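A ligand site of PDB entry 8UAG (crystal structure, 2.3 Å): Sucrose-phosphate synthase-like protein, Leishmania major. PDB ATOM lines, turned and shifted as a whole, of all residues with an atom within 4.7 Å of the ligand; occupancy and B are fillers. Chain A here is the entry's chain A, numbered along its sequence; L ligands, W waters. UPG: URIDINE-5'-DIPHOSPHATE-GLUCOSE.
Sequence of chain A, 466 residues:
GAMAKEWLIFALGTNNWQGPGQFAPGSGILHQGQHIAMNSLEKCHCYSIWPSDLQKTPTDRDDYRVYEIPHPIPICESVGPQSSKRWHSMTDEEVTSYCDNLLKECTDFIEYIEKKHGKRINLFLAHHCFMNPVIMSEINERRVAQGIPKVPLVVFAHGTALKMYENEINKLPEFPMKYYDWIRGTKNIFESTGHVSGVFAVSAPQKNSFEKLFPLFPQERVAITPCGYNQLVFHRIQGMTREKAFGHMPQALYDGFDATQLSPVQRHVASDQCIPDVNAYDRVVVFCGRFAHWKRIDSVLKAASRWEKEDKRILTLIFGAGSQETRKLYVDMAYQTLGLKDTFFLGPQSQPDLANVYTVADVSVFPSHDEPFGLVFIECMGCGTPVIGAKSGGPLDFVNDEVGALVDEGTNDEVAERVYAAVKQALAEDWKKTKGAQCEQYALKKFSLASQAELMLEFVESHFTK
O2C of the ligand lies within hydrogen-bond range of OE2 of Glu 379, at 2.5 Å. O4 of the ligand sits at hydrogen-bond distance from N of Gln 349, at 3.0 Å. The backbone carbonyl oxygen (O) of Gln 349 sits at hydrogen-bond distance from a nitrogen (N3) of the ligand (2.6 Å). OE2 of Glu 371 is in hydrogen-bond range of O3' of the ligand, 2.6 Å away. The backbone NH of Arg 290 is in hydrogen-bond range of an oxygen (O1A) of the ligand. The guanidinium group of Arg 290 is in salt-bridge range of an oxygen (O2B) of the ligand. The side-chain amino group (NZ) of Lys 295 is in salt-bridge range of an oxygen (O2A) of the ligand (2.8 Å). O2 of the ligand sits at hydrogen-bond distance from NE2 of Gln 18, 2.8 Å away. The side-chain amide nitrogen (NE2) of Gln 351 is in hydrogen-bond range of an oxygen (O2C) of the ligand. An oxygen (O1B) of the ligand is in hydrogen-bond range of the backbone NH (N) of Gly 26, at 3.0 Å. The backbone NH of Phe 373 is in hydrogen-bond range of an oxygen (O3') of the ligand, 3.0 Å away. An oxygen (O3') of the ligand is in hydrogen-bond range of the backbone NH (N) of Gly 374. N of Leu 375 is in hydrogen-bond range of O4' of the ligand, at 3.1 Å. The backbone NH of Val 376 sits close to an oxygen (O3C) of the ligand (3.4 Å).
The side-chain carboxylate of Glu 371 is in salt-bridge range of the side-chain amino group of Lys 295, 2.9 Å away. The backbone carbonyl oxygen of Gly 347 lies within hydrogen-bond range of the backbone NH of Gly 320, at 2.9 Å.
Residues that only touch the ligand: Pro 348 (3.2 Å), Gly 289 (3.3 Å), Pro 372 (3.4 Å), Leu 354 (3.4 Å), Cys 288 (3.6 Å), Trp 294 (3.6 Å), Ile 29 (3.6 Å), Gly 320 (3.8 Å) and Val 202 (3.9 Å). Hydrophobic or aromatic side chains that line the ligand: Ile 29, Val 202, Trp 294, Pro 348, Leu 354, Pro 372, Phe 373, Leu 375 and Val 376. The nearest printed residue that does not touch the ligand is Leu 30 (4.03 Å).
Water W3 lies within hydrogen-bond range of the backbone NH (N) of Leu 375 (2.9 Å), an oxygen (O2A) of the ligand (2.9 Å), the side-chain carboxylate (OE2) of Glu 371 (3.0 Å) and the backbone NH (N) of Val 376 (3.3 Å). Water W4 lies within hydrogen-bond range of OE1 of Gln 18 (2.7 Å) and N3 of the ligand (3.5 Å).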
ATOM      1  N   GLN A  18      15.315 -17.466 -20.177  1.00  0.00           N
ATOM      2  CA  GLN A  18      15.765 -18.592 -19.374  1.00  0.00           C
ATOM      3  C   GLN A  18      14.717 -18.900 -18.304  1.00  0.00           C
ATOM      4  O   GLN A  18      14.399 -18.045 -17.478  1.00  0.00           O
ATOM      5  CB  GLN A  18      17.112 -18.270 -18.753  1.00  0.00           C
ATOM      6  CG  GLN A  18      17.703 -19.382 -17.906  1.00  0.00           C
ATOM      7  CD  GLN A  18      19.198 -19.542 -18.135  1.00  0.00           C
ATOM      8  OE1 GLN A  18      19.640 -19.870 -19.244  1.00  0.00           O
ATOM      9  NE2 GLN A  18      19.981 -19.299 -17.088  1.00  0.00           N
ATOM     10  N   PHE A  23      17.073 -23.520 -20.967  1.00  0.00           N
ATOM     11  CA  PHE A  23      18.114 -22.518 -20.878  1.00  0.00           C
ATOM     12  C   PHE A  23      18.025 -21.585 -22.086  1.00  0.00           C
ATOM     13  O   PHE A  23      17.530 -21.960 -23.156  1.00  0.00           O
ATOM     14  CB  PHE A  23      19.460 -23.209 -20.744  1.00  0.00           C
ATOM     15  CG  PHE A  23      19.703 -23.777 -19.368  1.00  0.00           C
ATOM     16  CD1 PHE A  23      20.120 -22.966 -18.327  1.00  0.00           C
ATOM     17  CD2 PHE A  23      19.471 -25.121 -19.111  1.00  0.00           C
ATOM     18  CE1 PHE A  23      20.334 -23.472 -17.079  1.00  0.00           C
ATOM     19  CE2 PHE A  23      19.682 -25.619 -17.852  1.00  0.00           C
ATOM     20  CZ  PHE A  23      20.107 -24.797 -16.844  1.00  0.00           C
ATOM     21  N   PRO A  25      19.746 -18.967 -24.973  1.00  0.00           N
ATOM     22  CA  PRO A  25      20.977 -18.541 -25.639  1.00  0.00           C
ATOM     23  C   PRO A  25      21.350 -17.125 -25.230  1.00  0.00           C
ATOM     24  O   PRO A  25      20.570 -16.396 -24.618  1.00  0.00           O
ATOM     25  CB  PRO A  25      20.623 -18.609 -27.127  1.00  0.00           C
ATOM     26  CG  PRO A  25      19.127 -18.482 -27.157  1.00  0.00           C
ATOM     27  CD  PRO A  25      18.610 -19.087 -25.894  1.00  0.00           C
ATOM     28  N   GLY A  26      22.564 -16.705 -25.622  1.00  0.00           N
ATOM     29  CA  GLY A  26      23.014 -15.354 -25.326  1.00  0.00           C
ATOM     30  C   GLY A  26      21.997 -14.271 -25.714  1.00  0.00           C
ATOM     31  O   GLY A  26      21.740 -13.344 -24.937  1.00  0.00           O
ATOM     32  N   SER A  27      21.394 -14.410 -26.884  1.00  0.00           N
ATOM     33  CA  SER A  27      20.420 -13.442 -27.364  1.00  0.00           C
ATOM     34  C   SER A  27      19.243 -13.310 -26.403  1.00  0.00           C
ATOM     35  O   SER A  27      18.742 -12.204 -26.164  1.00  0.00           O
ATOM     36  CB  SER A  27      19.894 -13.875 -28.725  1.00  0.00           C
ATOM     37  OG  SER A  27      18.822 -13.017 -29.072  1.00  0.00           O
ATOM     38  N   ILE A  29      19.165 -14.173 -23.150  1.00  0.00           N
ATOM     39  CA  ILE A  29      19.651 -13.591 -21.905  1.00  0.00           C
ATOM     40  C   ILE A  29      19.705 -12.083 -22.034  1.00  0.00           C
ATOM     41  O   ILE A  29      19.324 -11.355 -21.126  1.00  0.00           O
ATOM     42  CB  ILE A  29      21.040 -14.167 -21.557  1.00  0.00           C
ATOM     43  CG1 ILE A  29      20.973 -15.649 -21.197  1.00  0.00           C
ATOM     44  CG2 ILE A  29      21.668 -13.346 -20.460  1.00  0.00           C
ATOM     45  CD1 ILE A  29      20.147 -15.984 -19.949  1.00  0.00           C
ATOM     46  N   LEU A  30      20.170 -11.590 -23.187  1.00  0.00           N
ATOM     47  CA  LEU A  30      20.309 -10.143 -23.337  1.00  0.00           C
ATOM     48  C   LEU A  30      18.958  -9.477 -23.335  1.00  0.00           C
ATOM     49  O   LEU A  30      18.779  -8.424 -22.717  1.00  0.00           O
ATOM     50  CB  LEU A  30      21.047  -9.823 -24.623  1.00  0.00           C
ATOM     51  CG  LEU A  30      21.270  -8.343 -24.932  1.00  0.00           C
ATOM     52  CD1 LEU A  30      22.389  -7.764 -24.078  1.00  0.00           C
ATOM     53  CD2 LEU A  30      21.618  -8.168 -26.399  1.00  0.00           C
ATOM     54  N   VAL A 202      25.895  -6.243 -31.389  1.00  0.00           N
ATOM     55  CA  VAL A 202      26.523  -6.634 -30.122  1.00  0.00           C
ATOM     56  C   VAL A 202      28.038  -6.550 -30.205  1.00  0.00           C
ATOM     57  O   VAL A 202      28.708  -6.390 -29.189  1.00  0.00           O
ATOM     58  CB  VAL A 202      26.107  -8.057 -29.689  1.00  0.00           C
ATOM     59  CG1 VAL A 202      26.889  -8.490 -28.432  1.00  0.00           C
ATOM     60  CG2 VAL A 202      24.599  -8.135 -29.390  1.00  0.00           C
ATOM     61  N   PHE A 234      23.938 -11.243  -9.697  1.00  0.00           N
ATOM     62  CA  PHE A 234      25.394 -11.407  -9.676  1.00  0.00           C
ATOM     63  C   PHE A 234      25.955 -10.354  -8.721  1.00  0.00           C
ATOM     64  O   PHE A 234      26.174  -9.208  -9.074  1.00  0.00           O
ATOM     65  CB  PHE A 234      25.979 -11.328 -11.081  1.00  0.00           C
ATOM     66  CG  PHE A 234      25.607 -12.501 -11.941  1.00  0.00           C
ATOM     67  CD1 PHE A 234      26.273 -13.713 -11.818  1.00  0.00           C
ATOM     68  CD2 PHE A 234      24.561 -12.421 -12.839  1.00  0.00           C
ATOM     69  CE1 PHE A 234      25.913 -14.805 -12.609  1.00  0.00           C
ATOM     70  CE2 PHE A 234      24.204 -13.507 -13.652  1.00  0.00           C
ATOM     71  CZ  PHE A 234      24.873 -14.691 -13.541  1.00  0.00           C
ATOM     72  N   CYS A 288      32.941 -20.886 -17.730  1.00  0.00           N
ATOM     73  CA  CYS A 288      31.516 -20.976 -18.003  1.00  0.00           C
ATOM     74  C   CYS A 288      31.336 -20.502 -19.435  1.00  0.00           C
ATOM     75  O   CYS A 288      31.897 -19.485 -19.837  1.00  0.00           O
ATOM     76  CB  CYS A 288      30.674 -20.140 -17.033  1.00  0.00           C
ATOM     77  SG  CYS A 288      28.908 -20.087 -17.486  1.00  0.00           S
ATOM     78  N   GLY A 289      30.602 -21.275 -20.215  1.00  0.00           N
ATOM     79  CA  GLY A 289      30.276 -20.878 -21.554  1.00  0.00           C
ATOM     80  C   GLY A 289      29.654 -22.042 -22.294  1.00  0.00           C
ATOM     81  O   GLY A 289      29.846 -23.187 -21.908  1.00  0.00           O
ATOM     82  N   ARG A 290      28.895 -21.748 -23.337  1.00  0.00           N
ATOM     83  CA  ARG A 290      28.444 -22.802 -24.219  1.00  0.00           C
ATOM     84  C   ARG A 290      29.637 -23.404 -24.967  1.00  0.00           C
ATOM     85  O   ARG A 290      30.631 -22.737 -25.252  1.00  0.00           O
ATOM     86  CB  ARG A 290      27.392 -22.278 -25.186  1.00  0.00           C
ATOM     87  CG  ARG A 290      27.929 -21.232 -26.173  1.00  0.00           C
ATOM     88  CD  ARG A 290      26.875 -20.880 -27.220  1.00  0.00           C
ATOM     89  NE  ARG A 290      27.191 -19.678 -27.974  1.00  0.00           N
ATOM     90  CZ  ARG A 290      27.327 -19.656 -29.287  1.00  0.00           C
ATOM     91  NH1 ARG A 290      27.280 -20.770 -30.008  1.00  0.00           N
ATOM     92  NH2 ARG A 290      27.481 -18.487 -29.902  1.00  0.00           N
ATOM     93  N   TRP A 294      34.988 -21.664 -30.703  1.00  0.00           N
ATOM     94  CA  TRP A 294      35.704 -20.420 -30.447  1.00  0.00           C
ATOM     95  C   TRP A 294      35.770 -20.034 -28.959  1.00  0.00           C
ATOM     96  O   TRP A 294      36.500 -19.096 -28.617  1.00  0.00           O
ATOM     97  CB  TRP A 294      35.082 -19.308 -31.274  1.00  0.00           C
ATOM     98  CG  TRP A 294      33.641 -19.066 -30.959  1.00  0.00           C
ATOM     99  CD1 TRP A 294      32.558 -19.554 -31.638  1.00  0.00           C
ATOM    100  CD2 TRP A 294      33.125 -18.274 -29.880  1.00  0.00           C
ATOM    101  NE1 TRP A 294      31.389 -19.117 -31.038  1.00  0.00           N
ATOM    102  CE2 TRP A 294      31.715 -18.323 -29.961  1.00  0.00           C
ATOM    103  CE3 TRP A 294      33.730 -17.518 -28.848  1.00  0.00           C
ATOM    104  CZ2 TRP A 294      30.895 -17.655 -29.067  1.00  0.00           C
ATOM    105  CZ3 TRP A 294      32.918 -16.858 -27.945  1.00  0.00           C
ATOM    106  CH2 TRP A 294      31.508 -16.939 -28.057  1.00  0.00           C
ATOM    107  N   LYS A 295      35.076 -20.734 -28.061  1.00  0.00           N
ATOM    108  CA  LYS A 295      35.270 -20.483 -26.636  1.00  0.00           C
ATOM    109  C   LYS A 295      36.604 -21.019 -26.160  1.00  0.00           C
ATOM    110  O   LYS A 295      37.086 -20.592 -25.097  1.00  0.00           O
ATOM    111  CB  LYS A 295      34.140 -21.110 -25.807  1.00  0.00           C
ATOM    112  CG  LYS A 295      32.820 -20.376 -25.877  1.00  0.00           C
ATOM    113  CD  LYS A 295      32.832 -19.078 -25.088  1.00  0.00           C
ATOM    114  CE  LYS A 295      31.415 -18.509 -24.982  1.00  0.00           C
ATOM    115  NZ  LYS A 295      31.371 -17.270 -24.135  1.00  0.00           N
ATOM    116  N   GLY A 320      28.317 -24.846 -18.398  1.00  0.00           N
ATOM    117  CA  GLY A 320      27.834 -24.542 -19.724  1.00  0.00           C
ATOM    118  C   GLY A 320      27.299 -25.745 -20.476  1.00  0.00           C
ATOM    119  O   GLY A 320      27.646 -26.885 -20.154  1.00  0.00           O
ATOM    120  N   GLY A 347      27.699 -28.830 -16.178  1.00  0.00           N
ATOM    121  CA  GLY A 347      26.522 -28.575 -16.972  1.00  0.00           C
ATOM    122  C   GLY A 347      26.129 -27.125 -16.998  1.00  0.00           C
ATOM    123  O   GLY A 347      26.780 -26.284 -16.384  1.00  0.00           O
ATOM    124  N   PRO A 348      25.052 -26.789 -17.727  1.00  0.00           N
ATOM    125  CA  PRO A 348      24.476 -25.456 -17.629  1.00  0.00           C
ATOM    126  C   PRO A 348      23.784 -25.247 -16.283  1.00  0.00           C
ATOM    127  O   PRO A 348      23.177 -26.151 -15.715  1.00  0.00           O
ATOM    128  CB  PRO A 348      23.457 -25.426 -18.782  1.00  0.00           C
ATOM    129  CG  PRO A 348      22.979 -26.876 -18.808  1.00  0.00           C
ATOM    130  CD  PRO A 348      24.219 -27.692 -18.560  1.00  0.00           C
ATOM    131  N   GLN A 349      23.873 -24.020 -15.793  1.00  0.00           N
ATOM    132  CA  GLN A 349      23.326 -23.696 -14.490  1.00  0.00           C
ATOM    133  C   GLN A 349      22.550 -22.382 -14.564  1.00  0.00           C
ATOM    134  O   GLN A 349      22.772 -21.561 -15.450  1.00  0.00           O
ATOM    135  CB  GLN A 349      24.437 -23.590 -13.426  1.00  0.00           C
ATOM    136  CG  GLN A 349      25.217 -24.878 -13.188  1.00  0.00           C
ATOM    137  CD  GLN A 349      24.423 -25.949 -12.503  1.00  0.00           C
ATOM    138  OE1 GLN A 349      23.385 -25.694 -11.894  1.00  0.00           O
ATOM    139  NE2 GLN A 349      24.901 -27.165 -12.609  1.00  0.00           N
ATOM    140  N   SER A 350      21.656 -22.194 -13.619  1.00  0.00           N
ATOM    141  CA  SER A 350      20.932 -20.949 -13.509  1.00  0.00           C
ATOM    142  C   SER A 350      21.865 -19.805 -13.093  1.00  0.00           C
ATOM    143  O   SER A 350      22.942 -19.985 -12.502  1.00  0.00           O
ATOM    144  CB  SER A 350      19.812 -21.082 -12.475  1.00  0.00           C
ATOM    145  OG  SER A 350      20.374 -21.077 -11.167  1.00  0.00           O
ATOM    146  N   GLN A 351      21.429 -18.599 -13.434  1.00  0.00           N
ATOM    147  CA  GLN A 351      22.190 -17.419 -13.044  1.00  0.00           C
ATOM    148  C   GLN A 351      22.424 -17.371 -11.543  1.00  0.00           C
ATOM    149  O   GLN A 351      23.579 -17.167 -11.136  1.00  0.00           O
ATOM    150  CB  GLN A 351      21.474 -16.185 -13.589  1.00  0.00           C
ATOM    151  CG  GLN A 351      21.567 -16.084 -15.120  1.00  0.00           C
ATOM    152  CD  GLN A 351      21.124 -14.740 -15.669  1.00  0.00           C
ATOM    153  OE1 GLN A 351      20.175 -14.127 -15.184  1.00  0.00           O
ATOM    154  NE2 GLN A 351      21.845 -14.260 -16.664  1.00  0.00           N
ATOM    155  N   LEU A 354      25.218 -19.653 -10.599  1.00  0.00           N
ATOM    156  CA  LEU A 354      26.545 -19.245 -11.063  1.00  0.00           C
ATOM    157  C   LEU A 354      27.089 -18.143 -10.177  1.00  0.00           C
ATOM    158  O   LEU A 354      28.298 -18.129  -9.874  1.00  0.00           O
ATOM    159  CB  LEU A 354      26.496 -18.790 -12.521  1.00  0.00           C
ATOM    160  CG  LEU A 354      26.430 -19.868 -13.611  1.00  0.00           C
ATOM    161  CD1 LEU A 354      25.861 -19.310 -14.918  1.00  0.00           C
ATOM    162  CD2 LEU A 354      27.788 -20.502 -13.865  1.00  0.00           C
ATOM    163  N   GLU A 371      35.492 -13.097 -28.465  1.00  0.00           N
ATOM    164  CA  GLU A 371      34.234 -13.031 -27.730  1.00  0.00           C
ATOM    165  C   GLU A 371      33.453 -11.802 -28.205  1.00  0.00           C
ATOM    166  O   GLU A 371      34.029 -10.711 -28.333  1.00  0.00           O
ATOM    167  CB  GLU A 371      34.486 -12.972 -26.224  1.00  0.00           C
ATOM    168  CG  GLU A 371      33.257 -12.873 -25.351  1.00  0.00           C
ATOM    169  CD  GLU A 371      32.589 -14.241 -25.089  1.00  0.00           C
ATOM    170  OE1 GLU A 371      33.304 -15.245 -24.859  1.00  0.00           O
ATOM    171  OE2 GLU A 371      31.350 -14.314 -25.071  1.00  0.00           O
ATOM    172  N   PRO A 372      32.187 -11.946 -28.541  1.00  0.00           N
ATOM    173  CA  PRO A 372      31.464 -10.789 -29.083  1.00  0.00           C
ATOM    174  C   PRO A 372      31.438  -9.658 -28.094  1.00  0.00           C
ATOM    175  O   PRO A 372      31.891  -8.549 -28.385  1.00  0.00           O
ATOM    176  CB  PRO A 372      30.073 -11.347 -29.387  1.00  0.00           C
ATOM    177  CG  PRO A 372      30.392 -12.791 -29.776  1.00  0.00           C
ATOM    178  CD  PRO A 372      31.480 -13.211 -28.779  1.00  0.00           C
ATOM    179  N   PHE A 373      30.905  -9.912 -26.896  1.00  0.00           N
ATOM    180  CA  PHE A 373      30.998  -8.933 -25.822  1.00  0.00           C
ATOM    181  C   PHE A 373      31.665  -9.513 -24.582  1.00  0.00           C
ATOM    182  O   PHE A 373      32.720  -9.025 -24.174  1.00  0.00           O
ATOM    183  CB  PHE A 373      29.633  -8.362 -25.440  1.00  0.00           C
ATOM    184  CG  PHE A 373      29.714  -7.449 -24.310  1.00  0.00           C
ATOM    185  CD1 PHE A 373      30.370  -6.243 -24.441  1.00  0.00           C
ATOM    186  CD2 PHE A 373      29.223  -7.816 -23.069  1.00  0.00           C
ATOM    187  CE1 PHE A 373      30.498  -5.386 -23.373  1.00  0.00           C
ATOM    188  CE2 PHE A 373      29.337  -6.969 -21.987  1.00  0.00           C
ATOM    189  CZ  PHE A 373      29.972  -5.753 -22.123  1.00  0.00           C
ATOM    190  N   GLY A 374      31.093 -10.566 -24.000  1.00  0.00           N
ATOM    191  CA  GLY A 374      31.653 -11.205 -22.833  1.00  0.00           C
ATOM    192  C   GLY A 374      30.854 -10.968 -21.573  1.00  0.00           C
ATOM    193  O   GLY A 374      31.374 -10.495 -20.563  1.00  0.00           O
ATOM    194  N   LEU A 375      29.563 -11.332 -21.618  1.00  0.00           N
ATOM    195  CA  LEU A 375      28.714 -11.200 -20.435  1.00  0.00           C
ATOM    196  C   LEU A 375      29.261 -11.985 -19.241  1.00  0.00           C
ATOM    197  O   LEU A 375      29.159 -11.535 -18.092  1.00  0.00           O
ATOM    198  CB  LEU A 375      27.317 -11.690 -20.811  1.00  0.00           C
ATOM    199  CG  LEU A 375      26.151 -11.349 -19.909  1.00  0.00           C
ATOM    200  CD1 LEU A 375      26.272  -9.913 -19.453  1.00  0.00           C
ATOM    201  CD2 LEU A 375      24.877 -11.580 -20.708  1.00  0.00           C
ATOM    202  N   VAL A 376      29.833 -13.163 -19.497  1.00  0.00           N
ATOM    203  CA  VAL A 376      30.372 -13.983 -18.415  1.00  0.00           C
ATOM    204  C   VAL A 376      31.443 -13.228 -17.644  1.00  0.00           C
ATOM    205  O   VAL A 376      31.518 -13.351 -16.418  1.00  0.00           O
ATOM    206  CB  VAL A 376      30.934 -15.316 -18.955  1.00  0.00           C
ATOM    207  CG1 VAL A 376      29.796 -16.133 -19.541  1.00  0.00           C
ATOM    208  CG2 VAL A 376      32.028 -15.092 -19.984  1.00  0.00           C
ATOM    209  N   GLU A 379      29.551 -10.593 -15.326  1.00  0.00           N
ATOM    210  CA  GLU A 379      28.899 -11.309 -14.232  1.00  0.00           C
ATOM    211  C   GLU A 379      29.912 -11.762 -13.182  1.00  0.00           C
ATOM    212  O   GLU A 379      29.693 -11.590 -11.986  1.00  0.00           O
ATOM    213  CB  GLU A 379      28.101 -12.500 -14.777  1.00  0.00           C
ATOM    214  CG  GLU A 379      26.856 -12.105 -15.597  1.00  0.00           C
ATOM    215  CD  GLU A 379      26.330 -13.204 -16.499  1.00  0.00           C
ATOM    216  OE1 GLU A 379      27.033 -14.234 -16.680  1.00  0.00           O
ATOM    217  OE2 GLU A 379      25.191 -13.043 -17.000  1.00  0.00           O
HETATM  218  N1  UPG L   1      24.421 -18.446 -18.939  1.00  0.00           N
HETATM  219  C2  UPG L   1      23.552 -19.092 -17.818  1.00  0.00           C
HETATM  220  N3  UPG L   1      23.938 -20.535 -17.489  1.00  0.00           N
HETATM  221  C4  UPG L   1      25.028 -21.229 -18.167  1.00  0.00           C
HETATM  222  C5  UPG L   1      25.782 -20.577 -19.194  1.00  0.00           C
HETATM  223  C6  UPG L   1      25.483 -19.212 -19.586  1.00  0.00           C
HETATM  224  O2  UPG L   1      22.685 -18.478 -17.304  1.00  0.00           O
HETATM  225  O4  UPG L   1      25.268 -22.380 -17.846  1.00  0.00           O
HETATM  226  C1C UPG L   1      24.126 -17.199 -19.257  1.00  0.00           C
HETATM  227  C2C UPG L   1      25.124 -16.209 -18.513  1.00  0.00           C
HETATM  228  O2C UPG L   1      24.316 -15.039 -18.130  1.00  0.00           O
HETATM  229  C3C UPG L   1      26.022 -15.974 -19.364  1.00  0.00           C
HETATM  230  C4C UPG L   1      25.160 -15.869 -20.790  1.00  0.00           C
HETATM  231  O4C UPG L   1      24.338 -16.893 -20.742  1.00  0.00           O
HETATM  232  O3C UPG L   1      26.765 -14.716 -19.240  1.00  0.00           O
HETATM  233  C5C UPG L   1      26.095 -15.877 -21.937  1.00  0.00           C
HETATM  234  O5C UPG L   1      26.807 -17.067 -21.910  1.00  0.00           O
HETATM  235  PA  UPG L   1      27.598 -17.578 -23.307  1.00  0.00           P
HETATM  236  O1A UPG L   1      28.092 -19.027 -23.101  1.00  0.00           O
HETATM  237  O2A UPG L   1      28.660 -16.598 -23.679  1.00  0.00           O
HETATM  238  O3A UPG L   1      26.501 -17.661 -24.530  1.00  0.00           O
HETATM  239  PB  UPG L   1      26.585 -16.859 -25.938  1.00  0.00           P
HETATM  240  O1B UPG L   1      25.321 -17.236 -26.622  1.00  0.00           O
HETATM  241  O2B UPG L   1      27.811 -17.263 -26.741  1.00  0.00           O
HETATM  242  O3B UPG L   1      26.637 -15.219 -25.613  1.00  0.00           O
HETATM  243  C1' UPG L   1      26.502 -14.282 -26.663  1.00  0.00           C
HETATM  244  C2' UPG L   1      27.876 -13.694 -26.915  1.00  0.00           C
HETATM  245  C3' UPG L   1      28.360 -12.967 -25.673  1.00  0.00           C
HETATM  246  C4' UPG L   1      27.397 -11.903 -25.349  1.00  0.00           C
HETATM  247  C5' UPG L   1      25.998 -12.449 -25.080  1.00  0.00           C
HETATM  248  C6' UPG L   1      25.002 -11.333 -24.832  1.00  0.00           C
HETATM  249  O2' UPG L   1      28.757 -14.766 -27.237  1.00  0.00           O
HETATM  250  O3' UPG L   1      29.710 -12.486 -25.968  1.00  0.00           O
HETATM  251  O4' UPG L   1      27.822 -11.156 -24.174  1.00  0.00           O
HETATM  252  O5' UPG L   1      25.527 -13.315 -26.230  1.00  0.00           O
HETATM  253  O6' UPG L   1      24.710 -10.742 -26.101  1.00  0.00           O
HETATM  254  O   HOH W   1      23.874 -11.746 -28.507  1.00  0.00           O
HETATM  255  O   HOH W   2      25.531 -20.443 -23.110  1.00  0.00           O
HETATM  256  O   HOH W   3      29.521 -13.992 -22.713  1.00  0.00           O
HETATM  257  O   HOH W   4      22.088 -20.263 -20.412  1.00  0.00           O
HETATM  258  O   HOH W   5      23.485 -18.638 -22.671  1.00  0.00           O
